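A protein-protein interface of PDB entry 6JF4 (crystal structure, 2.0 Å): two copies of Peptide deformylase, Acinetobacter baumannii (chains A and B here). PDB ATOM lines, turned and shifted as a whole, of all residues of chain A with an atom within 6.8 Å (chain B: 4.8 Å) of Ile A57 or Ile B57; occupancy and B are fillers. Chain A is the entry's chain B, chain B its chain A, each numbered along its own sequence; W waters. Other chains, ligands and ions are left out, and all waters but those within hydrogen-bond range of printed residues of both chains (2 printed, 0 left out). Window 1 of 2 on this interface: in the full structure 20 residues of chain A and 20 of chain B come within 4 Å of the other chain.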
ATOM      1  N   LEU A   4     -21.305  -2.596   6.099  1.00  0.00           N
ATOM      2  CA  LEU A   4     -20.828  -1.621   7.121  1.00  0.00           C
ATOM      3  C   LEU A   4     -20.196  -0.433   6.418  1.00  0.00           C
ATOM      4  O   LEU A   4     -19.683  -0.581   5.311  1.00  0.00           O
ATOM      5  CB  LEU A   4     -19.785  -2.309   8.000  1.00  0.00           C
ATOM      6  CG  LEU A   4     -20.233  -3.515   8.820  1.00  0.00           C
ATOM      7  CD1 LEU A   4     -19.032  -4.140   9.510  1.00  0.00           C
ATOM      8  CD2 LEU A   4     -21.247  -3.112   9.852  1.00  0.00           C
ATOM      9  N   ILE A  13      -8.308   5.708  12.373  1.00  0.00           N
ATOM     10  CA  ILE A  13      -8.606   4.274  12.667  1.00  0.00           C
ATOM     11  C   ILE A  13      -7.701   3.392  11.794  1.00  0.00           C
ATOM     12  O   ILE A  13      -7.297   2.307  12.248  1.00  0.00           O
ATOM     13  CB  ILE A  13     -10.113   3.961  12.485  1.00  0.00           C
ATOM     14  CG1 ILE A  13     -10.498   2.585  13.036  1.00  0.00           C
ATOM     15  CG2 ILE A  13     -10.558   4.062  11.028  1.00  0.00           C
ATOM     16  CD1 ILE A  13     -10.147   2.386  14.450  1.00  0.00           C
ATOM     17  N   ALA A  18      -3.986  -2.924  15.204  1.00  0.00           N
ATOM     18  CA  ALA A  18      -5.227  -3.589  15.661  1.00  0.00           C
ATOM     19  C   ALA A  18      -4.911  -4.588  16.785  1.00  0.00           C
ATOM     20  O   ALA A  18      -3.780  -5.187  16.833  1.00  0.00           O
ATOM     21  CB  ALA A  18      -5.875  -4.254  14.472  1.00  0.00           C
ATOM     22  N   TRP A  30     -20.749 -13.448  18.307  1.00  0.00           N
ATOM     23  CA  TRP A  30     -20.111 -12.125  18.154  1.00  0.00           C
ATOM     24  C   TRP A  30     -19.072 -12.203  17.026  1.00  0.00           C
ATOM     25  O   TRP A  30     -19.148 -11.422  16.080  1.00  0.00           O
ATOM     26  CB  TRP A  30     -19.507 -11.707  19.494  1.00  0.00           C
ATOM     27  CG  TRP A  30     -18.291 -10.864  19.314  1.00  0.00           C
ATOM     28  CD1 TRP A  30     -16.996 -11.264  19.448  1.00  0.00           C
ATOM     29  CD2 TRP A  30     -18.251  -9.503  18.873  1.00  0.00           C
ATOM     30  NE1 TRP A  30     -16.149 -10.235  19.159  1.00  0.00           N
ATOM     31  CE2 TRP A  30     -16.886  -9.137  18.824  1.00  0.00           C
ATOM     32  CE3 TRP A  30     -19.224  -8.555  18.549  1.00  0.00           C
ATOM     33  CZ2 TRP A  30     -16.466  -7.865  18.436  1.00  0.00           C
ATOM     34  CZ3 TRP A  30     -18.812  -7.303  18.160  1.00  0.00           C
ATOM     35  CH2 TRP A  30     -17.453  -6.965  18.103  1.00  0.00           C
ATOM     36  N   LEU A  34     -19.385 -10.527  13.209  1.00  0.00           N
ATOM     37  CA  LEU A  34     -18.338  -9.570  12.737  1.00  0.00           C
ATOM     38  C   LEU A  34     -17.838 -10.006  11.358  1.00  0.00           C
ATOM     39  O   LEU A  34     -17.824  -9.188  10.437  1.00  0.00           O
ATOM     40  CB  LEU A  34     -17.188  -9.467  13.744  1.00  0.00           C
ATOM     41  CG  LEU A  34     -15.916  -8.813  13.184  1.00  0.00           C
ATOM     42  CD1 LEU A  34     -16.204  -7.359  12.879  1.00  0.00           C
ATOM     43  CD2 LEU A  34     -14.764  -8.936  14.146  1.00  0.00           C
ATOM     44  N   MET A  38     -18.294  -8.128   7.675  1.00  0.00           N
ATOM     45  CA  MET A  38     -17.073  -7.846   6.899  1.00  0.00           C
ATOM     46  C   MET A  38     -17.190  -8.485   5.509  1.00  0.00           C
ATOM     47  O   MET A  38     -16.795  -7.838   4.528  1.00  0.00           O
ATOM     48  CB  MET A  38     -15.817  -8.380   7.591  1.00  0.00           C
ATOM     49  CG  MET A  38     -15.422  -7.570   8.811  1.00  0.00           C
ATOM     50  SD  MET A  38     -14.000  -8.270   9.686  1.00  0.00           S
ATOM     51  CE  MET A  38     -12.724  -8.235   8.432  1.00  0.00           C
ATOM     52  N   ALA A  51     -10.143  -6.007   5.954  1.00  0.00           N
ATOM     53  CA  ALA A  51      -9.548  -6.056   7.289  1.00  0.00           C
ATOM     54  C   ALA A  51     -10.454  -5.272   8.222  1.00  0.00           C
ATOM     55  O   ALA A  51     -10.939  -4.248   7.808  1.00  0.00           O
ATOM     56  CB  ALA A  51      -8.160  -5.481   7.228  1.00  0.00           C
ATOM     57  N   ALA A  52     -10.578  -5.714   9.461  1.00  0.00           N
ATOM     58  CA  ALA A  52     -11.547  -5.178  10.431  1.00  0.00           C
ATOM     59  C   ALA A  52     -11.344  -3.680  10.617  1.00  0.00           C
ATOM     60  O   ALA A  52     -12.342  -2.972  10.699  1.00  0.00           O
ATOM     61  CB  ALA A  52     -11.470  -5.973  11.710  1.00  0.00           C
ATOM     62  N   PRO A  53     -10.102  -3.122  10.631  1.00  0.00           N
ATOM     63  CA  PRO A  53      -9.921  -1.683  10.811  1.00  0.00           C
ATOM     64  C   PRO A  53     -10.696  -0.845   9.790  1.00  0.00           C
ATOM     65  O   PRO A  53     -11.112   0.224  10.146  1.00  0.00           O
ATOM     66  CB  PRO A  53      -8.393  -1.494  10.693  1.00  0.00           C
ATOM     67  CG  PRO A  53      -7.846  -2.769  11.210  1.00  0.00           C
ATOM     68  CD  PRO A  53      -8.800  -3.814  10.649  1.00  0.00           C
ATOM     69  N   GLN A  54     -10.881  -1.357   8.574  1.00  0.00           N
ATOM     70  CA  GLN A  54     -11.528  -0.652   7.439  1.00  0.00           C
ATOM     71  C   GLN A  54     -13.007  -0.435   7.727  1.00  0.00           C
ATOM     72  O   GLN A  54     -13.598   0.434   7.043  1.00  0.00           O
ATOM     73  CB  GLN A  54     -11.420  -1.425   6.138  1.00  0.00           C
ATOM     74  CG  GLN A  54      -9.992  -1.562   5.638  1.00  0.00           C
ATOM     75  CD  GLN A  54      -9.929  -2.286   4.318  1.00  0.00           C
ATOM     76  OE1 GLN A  54      -9.815  -3.523   4.285  1.00  0.00           O
ATOM     77  NE2 GLN A  54     -10.045  -1.518   3.227  1.00  0.00           N
ATOM     78  N   VAL A  55     -13.574  -1.190   8.679  1.00  0.00           N
ATOM     79  CA  VAL A  55     -14.973  -1.033   9.151  1.00  0.00           C
ATOM     80  C   VAL A  55     -14.981  -0.581  10.619  1.00  0.00           C
ATOM     81  O   VAL A  55     -16.008  -0.776  11.305  1.00  0.00           O
ATOM     82  CB  VAL A  55     -15.796  -2.302   8.852  1.00  0.00           C
ATOM     83  CG1 VAL A  55     -15.847  -2.581   7.357  1.00  0.00           C
ATOM     84  CG2 VAL A  55     -15.304  -3.537   9.568  1.00  0.00           C
ATOM     85  N   TYR A  56     -13.910   0.097  11.058  1.00  0.00           N
ATOM     86  CA  TYR A  56     -13.802   0.804  12.354  1.00  0.00           C
ATOM     87  C   TYR A  56     -13.706  -0.188  13.519  1.00  0.00           C
ATOM     88  O   TYR A  56     -13.974   0.205  14.710  1.00  0.00           O
ATOM     89  CB  TYR A  56     -14.974   1.762  12.551  1.00  0.00           C
ATOM     90  CG  TYR A  56     -15.034   2.883  11.540  1.00  0.00           C
ATOM     91  CD1 TYR A  56     -14.324   4.055  11.736  1.00  0.00           C
ATOM     92  CD2 TYR A  56     -15.772   2.760  10.380  1.00  0.00           C
ATOM     93  CE1 TYR A  56     -14.376   5.102  10.821  1.00  0.00           C
ATOM     94  CE2 TYR A  56     -15.821   3.788   9.451  1.00  0.00           C
ATOM     95  CZ  TYR A  56     -15.118   4.956   9.664  1.00  0.00           C
ATOM     96  OH  TYR A  56     -15.149   5.976   8.743  1.00  0.00           O
ATOM     97  N   ILE A  57     -13.279  -1.415  13.226  1.00  0.00           N
ATOM     98  CA  ILE A  57     -13.055  -2.453  14.266  1.00  0.00           C
ATOM     99  C   ILE A  57     -11.551  -2.702  14.383  1.00  0.00           C
ATOM    100  O   ILE A  57     -10.969  -3.357  13.456  1.00  0.00           O
ATOM    101  CB  ILE A  57     -13.827  -3.722  13.918  1.00  0.00           C
ATOM    102  CG1 ILE A  57     -15.307  -3.443  13.628  1.00  0.00           C
ATOM    103  CG2 ILE A  57     -13.633  -4.765  14.988  1.00  0.00           C
ATOM    104  CD1 ILE A  57     -16.159  -3.139  14.812  1.00  0.00           C
ATOM    105  N   SER A  58     -10.928  -2.177  15.433  1.00  0.00           N
ATOM    106  CA  SER A  58      -9.454  -2.257  15.605  1.00  0.00           C
ATOM    107  C   SER A  58      -9.069  -3.609  16.214  1.00  0.00           C
ATOM    108  O   SER A  58      -8.522  -3.636  17.311  1.00  0.00           O
ATOM    109  CB  SER A  58      -8.914  -1.091  16.392  1.00  0.00           C
ATOM    110  OG  SER A  58      -7.516  -0.932  16.114  1.00  0.00           O
ATOM    111  N   LYS A  59      -9.328  -4.675  15.470  1.00  0.00           N
ATOM    112  CA  LYS A  59      -9.163  -6.092  15.856  1.00  0.00           C
ATOM    113  C   LYS A  59      -8.494  -6.837  14.699  1.00  0.00           C
ATOM    114  O   LYS A  59      -8.777  -6.503  13.537  1.00  0.00           O
ATOM    115  CB  LYS A  59     -10.523  -6.730  16.153  1.00  0.00           C
ATOM    116  CG  LYS A  59     -11.296  -6.186  17.357  1.00  0.00           C
ATOM    117  CD  LYS A  59     -10.512  -6.133  18.650  1.00  0.00           C
ATOM    118  CE  LYS A  59     -10.235  -7.471  19.295  1.00  0.00           C
ATOM    119  NZ  LYS A  59     -11.247  -7.748  20.322  1.00  0.00           N
ATOM    120  N   ARG A  60      -7.732  -7.884  15.018  1.00  0.00           N
ATOM    121  CA  ARG A  60      -6.927  -8.637  14.024  1.00  0.00           C
ATOM    122  C   ARG A  60      -7.770  -9.735  13.366  1.00  0.00           C
ATOM    123  O   ARG A  60      -7.566 -10.940  13.645  1.00  0.00           O
ATOM    124  CB  ARG A  60      -5.636  -9.121  14.679  1.00  0.00           C
ATOM    125  CG  ARG A  60      -4.837  -7.997  15.347  1.00  0.00           C
ATOM    126  CD  ARG A  60      -3.415  -8.324  15.804  1.00  0.00           C
ATOM    127  NE  ARG A  60      -2.464  -8.428  14.689  1.00  0.00           N
ATOM    128  CZ  ARG A  60      -1.886  -7.418  14.052  1.00  0.00           C
ATOM    129  NH1 ARG A  60      -2.130  -6.161  14.406  1.00  0.00           N
ATOM    130  NH2 ARG A  60      -1.044  -7.664  13.064  1.00  0.00           N
ATOM    131  N   VAL A  61      -8.685  -9.318  12.500  1.00  0.00           N
ATOM    132  CA  VAL A  61      -9.482 -10.210  11.621  1.00  0.00           C
ATOM    133  C   VAL A  61      -9.355  -9.725  10.193  1.00  0.00           C
ATOM    134  O   VAL A  61      -9.554  -8.525   9.977  1.00  0.00           O
ATOM    135  CB  VAL A  61     -10.950 -10.239  12.061  1.00  0.00           C
ATOM    136  CG1 VAL A  61     -11.754 -11.222  11.214  1.00  0.00           C
ATOM    137  CG2 VAL A  61     -11.071 -10.513  13.538  1.00  0.00           C
ATOM    138  N   LEU A 149      -3.848  -4.237   9.428  1.00  0.00           N
ATOM    139  CA  LEU A 149      -3.845  -4.550  10.876  1.00  0.00           C
ATOM    140  C   LEU A 149      -2.712  -3.801  11.573  1.00  0.00           C
ATOM    141  O   LEU A 149      -2.811  -3.619  12.792  1.00  0.00           O
ATOM    142  CB  LEU A 149      -3.680  -6.054  11.074  1.00  0.00           C
ATOM    143  CG  LEU A 149      -4.763  -6.957  10.505  1.00  0.00           C
ATOM    144  CD1 LEU A 149      -4.615  -8.357  11.109  1.00  0.00           C
ATOM    145  CD2 LEU A 149      -6.155  -6.414  10.759  1.00  0.00           C
ATOM    146  N   TRP B  30     -25.684  -8.074  13.809  1.00  0.00           N
ATOM    147  CA  TRP B  30     -24.365  -7.455  14.083  1.00  0.00           C
ATOM    148  C   TRP B  30     -24.501  -6.486  15.269  1.00  0.00           C
ATOM    149  O   TRP B  30     -23.767  -6.606  16.261  1.00  0.00           O
ATOM    150  CB  TRP B  30     -23.813  -6.792  12.809  1.00  0.00           C
ATOM    151  CG  TRP B  30     -22.930  -5.625  13.093  1.00  0.00           C
ATOM    152  CD1 TRP B  30     -23.212  -4.321  12.821  1.00  0.00           C
ATOM    153  CD2 TRP B  30     -21.660  -5.623  13.774  1.00  0.00           C
ATOM    154  NE1 TRP B  30     -22.193  -3.518  13.246  1.00  0.00           N
ATOM    155  CE2 TRP B  30     -21.234  -4.278  13.840  1.00  0.00           C
ATOM    156  CE3 TRP B  30     -20.841  -6.613  14.322  1.00  0.00           C
ATOM    157  CZ2 TRP B  30     -20.035  -3.898  14.436  1.00  0.00           C
ATOM    158  CZ3 TRP B  30     -19.660  -6.240  14.925  1.00  0.00           C
ATOM    159  CH2 TRP B  30     -19.266  -4.900  14.984  1.00  0.00           C
ATOM    160  N   LEU B  34     -22.968  -6.761  19.084  1.00  0.00           N
ATOM    161  CA  LEU B  34     -22.109  -5.686  19.637  1.00  0.00           C
ATOM    162  C   LEU B  34     -22.671  -5.209  20.973  1.00  0.00           C
ATOM    163  O   LEU B  34     -21.882  -5.150  21.924  1.00  0.00           O
ATOM    164  CB  LEU B  34     -21.928  -4.518  18.661  1.00  0.00           C
ATOM    165  CG  LEU B  34     -21.174  -3.323  19.261  1.00  0.00           C
ATOM    166  CD1 LEU B  34     -19.762  -3.699  19.642  1.00  0.00           C
ATOM    167  CD2 LEU B  34     -21.148  -2.138  18.316  1.00  0.00           C
ATOM    168  N   ALA B  52     -18.155   1.838  23.099  1.00  0.00           N
ATOM    169  CA  ALA B  52     -17.554   0.942  22.082  1.00  0.00           C
ATOM    170  C   ALA B  52     -16.051   1.167  21.905  1.00  0.00           C
ATOM    171  O   ALA B  52     -15.298   0.185  21.738  1.00  0.00           O
ATOM    172  CB  ALA B  52     -18.332   1.027  20.808  1.00  0.00           C
ATOM    173  N   PRO B  53     -15.523   2.416  21.864  1.00  0.00           N
ATOM    174  CA  PRO B  53     -14.076   2.588  21.746  1.00  0.00           C
ATOM    175  C   PRO B  53     -13.262   1.826  22.806  1.00  0.00           C
ATOM    176  O   PRO B  53     -12.143   1.396  22.505  1.00  0.00           O
ATOM    177  CB  PRO B  53     -13.901   4.092  21.886  1.00  0.00           C
ATOM    178  CG  PRO B  53     -15.185   4.624  21.287  1.00  0.00           C
ATOM    179  CD  PRO B  53     -16.251   3.693  21.812  1.00  0.00           C
ATOM    180  N   VAL B  55     -13.704  -1.127  23.849  1.00  0.00           N
ATOM    181  CA  VAL B  55     -13.535  -2.540  23.389  1.00  0.00           C
ATOM    182  C   VAL B  55     -13.079  -2.558  21.923  1.00  0.00           C
ATOM    183  O   VAL B  55     -13.388  -3.527  21.230  1.00  0.00           O
ATOM    184  CB  VAL B  55     -14.794  -3.376  23.680  1.00  0.00           C
ATOM    185  CG1 VAL B  55     -15.005  -3.472  25.179  1.00  0.00           C
ATOM    186  CG2 VAL B  55     -16.049  -2.851  22.999  1.00  0.00           C
ATOM    187  N   TYR B  56     -12.304  -1.530  21.522  1.00  0.00           N
ATOM    188  CA  TYR B  56     -11.596  -1.397  20.216  1.00  0.00           C
ATOM    189  C   TYR B  56     -12.553  -1.319  19.034  1.00  0.00           C
ATOM    190  O   TYR B  56     -12.150  -1.631  17.905  1.00  0.00           O
ATOM    191  CB  TYR B  56     -10.643  -2.571  19.985  1.00  0.00           C
ATOM    192  CG  TYR B  56      -9.521  -2.676  20.982  1.00  0.00           C
ATOM    193  CD1 TYR B  56      -8.350  -1.975  20.781  1.00  0.00           C
ATOM    194  CD2 TYR B  56      -9.625  -3.473  22.120  1.00  0.00           C
ATOM    195  CE1 TYR B  56      -7.305  -2.067  21.685  1.00  0.00           C
ATOM    196  CE2 TYR B  56      -8.580  -3.582  23.031  1.00  0.00           C
ATOM    197  CZ  TYR B  56      -7.414  -2.876  22.800  1.00  0.00           C
ATOM    198  OH  TYR B  56      -6.352  -2.909  23.652  1.00  0.00           O
ATOM    199  N   ILE B  57     -13.776  -0.886  19.278  1.00  0.00           N
ATOM    200  CA  ILE B  57     -14.812  -0.641  18.245  1.00  0.00           C
ATOM    201  C   ILE B  57     -15.008   0.884  18.141  1.00  0.00           C
ATOM    202  O   ILE B  57     -15.615   1.454  19.081  1.00  0.00           O
ATOM    203  CB  ILE B  57     -16.131  -1.327  18.630  1.00  0.00           C
ATOM    204  CG1 ILE B  57     -16.002  -2.800  19.040  1.00  0.00           C
ATOM    205  CG2 ILE B  57     -17.158  -1.110  17.535  1.00  0.00           C
ATOM    206  CD1 ILE B  57     -15.498  -3.680  17.977  1.00  0.00           C
ATOM    207  N   SER B  58     -14.535   1.536  17.065  1.00  0.00           N
ATOM    208  CA  SER B  58     -14.617   3.008  16.910  1.00  0.00           C
ATOM    209  C   SER B  58     -15.980   3.407  16.318  1.00  0.00           C
ATOM    210  O   SER B  58     -16.054   3.908  15.182  1.00  0.00           O
ATOM    211  CB  SER B  58     -13.424   3.533  16.146  1.00  0.00           C
ATOM    212  OG  SER B  58     -13.210   4.901  16.455  1.00  0.00           O
ATOM    213  N   LYS B  59     -17.039   3.116  17.060  1.00  0.00           N
ATOM    214  CA  LYS B  59     -18.446   3.399  16.704  1.00  0.00           C
ATOM    215  C   LYS B  59     -19.152   4.093  17.882  1.00  0.00           C
ATOM    216  O   LYS B  59     -18.803   3.804  19.052  1.00  0.00           O
ATOM    217  CB  LYS B  59     -19.138   2.098  16.280  1.00  0.00           C
ATOM    218  CG  LYS B  59     -18.647   1.614  14.920  1.00  0.00           C
ATOM    219  CD  LYS B  59     -19.438   0.518  14.291  1.00  0.00           C
ATOM    220  CE  LYS B  59     -19.397   0.569  12.778  1.00  0.00           C
ATOM    221  NZ  LYS B  59     -19.861   1.889  12.270  1.00  0.00           N
HETATM  222  O   HOH W   1     -18.151  -0.015   9.955  1.00  0.00           O
HETATM  223  O   HOH W   2     -12.120  -5.972  22.261  1.00  0.00           O
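O of Tyr A56 lies within hydrogen-bond range of N of Ser B58 (2.8 Å). O of Tyr B56 is in hydrogen-bond range of N of Ser A58 (2.8 Å).
The backbone carbonyl oxygen (O) of Ala A52 is in hydrogen-bond range of the backbone NH (N) of Ile A57 (3.1 Å). The backbone carbonyl oxygen (O) of Ala B52 is in hydrogen-bond range of the backbone NH (N) of Ile B57.
NE1 of Trp B30 touches CD2 of Leu A4, at 3.5 Å. Ser B58 touches Ile A13 (CB to CD1, 3.9 Å). Trp A30 touches Trp B30. Trp A30 touches Leu B34. Lys B59 touches Val A55 (CE to O, 3.9 Å). Tyr A56 touches Ile B57. CH2 of Trp B30 touches CD1 of Ile A57, at 3.6 Å. Ile A57 touches Tyr B56. Ile B57 touches Ile A57. CB of Tyr B56 touches CD of Lys A59, at 3.8 Å.
Printed residues of chain B within 4 Å of Leu A4: Trp B30 (3.5 Å). Printed residues of chain B within 4 Å of Val A55: Lys B59 (3.9 Å). Printed residues of chain B within 4 Å of Tyr A56: Ile B57 (3.6 Å) and Ser B58 (2.8 Å). Of chain B, only Trp B30, Tyr B56 and Ile B57 come within 4 Å of Ile A57. Printed residues of chain A within 4 Å of Trp B30: Leu A4 (3.5 Å), Trp A30 (3.5 Å) and Ile A57 (3.6 Å). Ala B52 touches none of the printed residues of chain A. Of chain A, only Trp A30 (3.8 Å), Tyr A56 (3.6 Å) and Ile A57 (3.3 Å) come within 4 Å of Ile B57. The nearest printed residue of chain B that does not touch Ile A57 is Lys B59 (4.9 Å). The nearest printed residue of chain A that does not touch Ile B57 is Lys A59 (4.9 Å). The nearest printed residue of chain A that does not touch Trp B30 is Leu A34 (4.2 Å).
Printed residues of chain B that touch a printed residue of chain A: Trp B30, Leu B34, Tyr B56, Ile B57, Ser B58 and Lys B59. Printed residues of chain A that touch a printed residue of chain B: Leu A4, Ile A13, Trp A30, Val A55, Tyr A56, Ile A57, Ser A58 and Lys A59. Among the printed residues, 13 pairs touch across the chains.
Trp A30 touches Leu B34, but with the chains exchanged Leu A34 does not touch Trp B30 (4.2 Å). Trp A30 touches Ile B57, and with the chains exchanged Ile A57 touches Trp B30. Val A55 touches Lys B59, but with the chains exchanged Lys A59 does not touch Val B55 (4.7 Å). Lys A59 touches Tyr B56, but with the chains exchanged Tyr A56 does not touch Lys B59 (4.4 Å). 9 positions are printed for both chains.
Water W1 bridges O of Val A55 (2.6 Å) and NZ of Lys B59 (3.5 Å). Water W2 bridges NZ of Lys A59 (2.8 Å) and O of Val B55 (2.9 Å).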
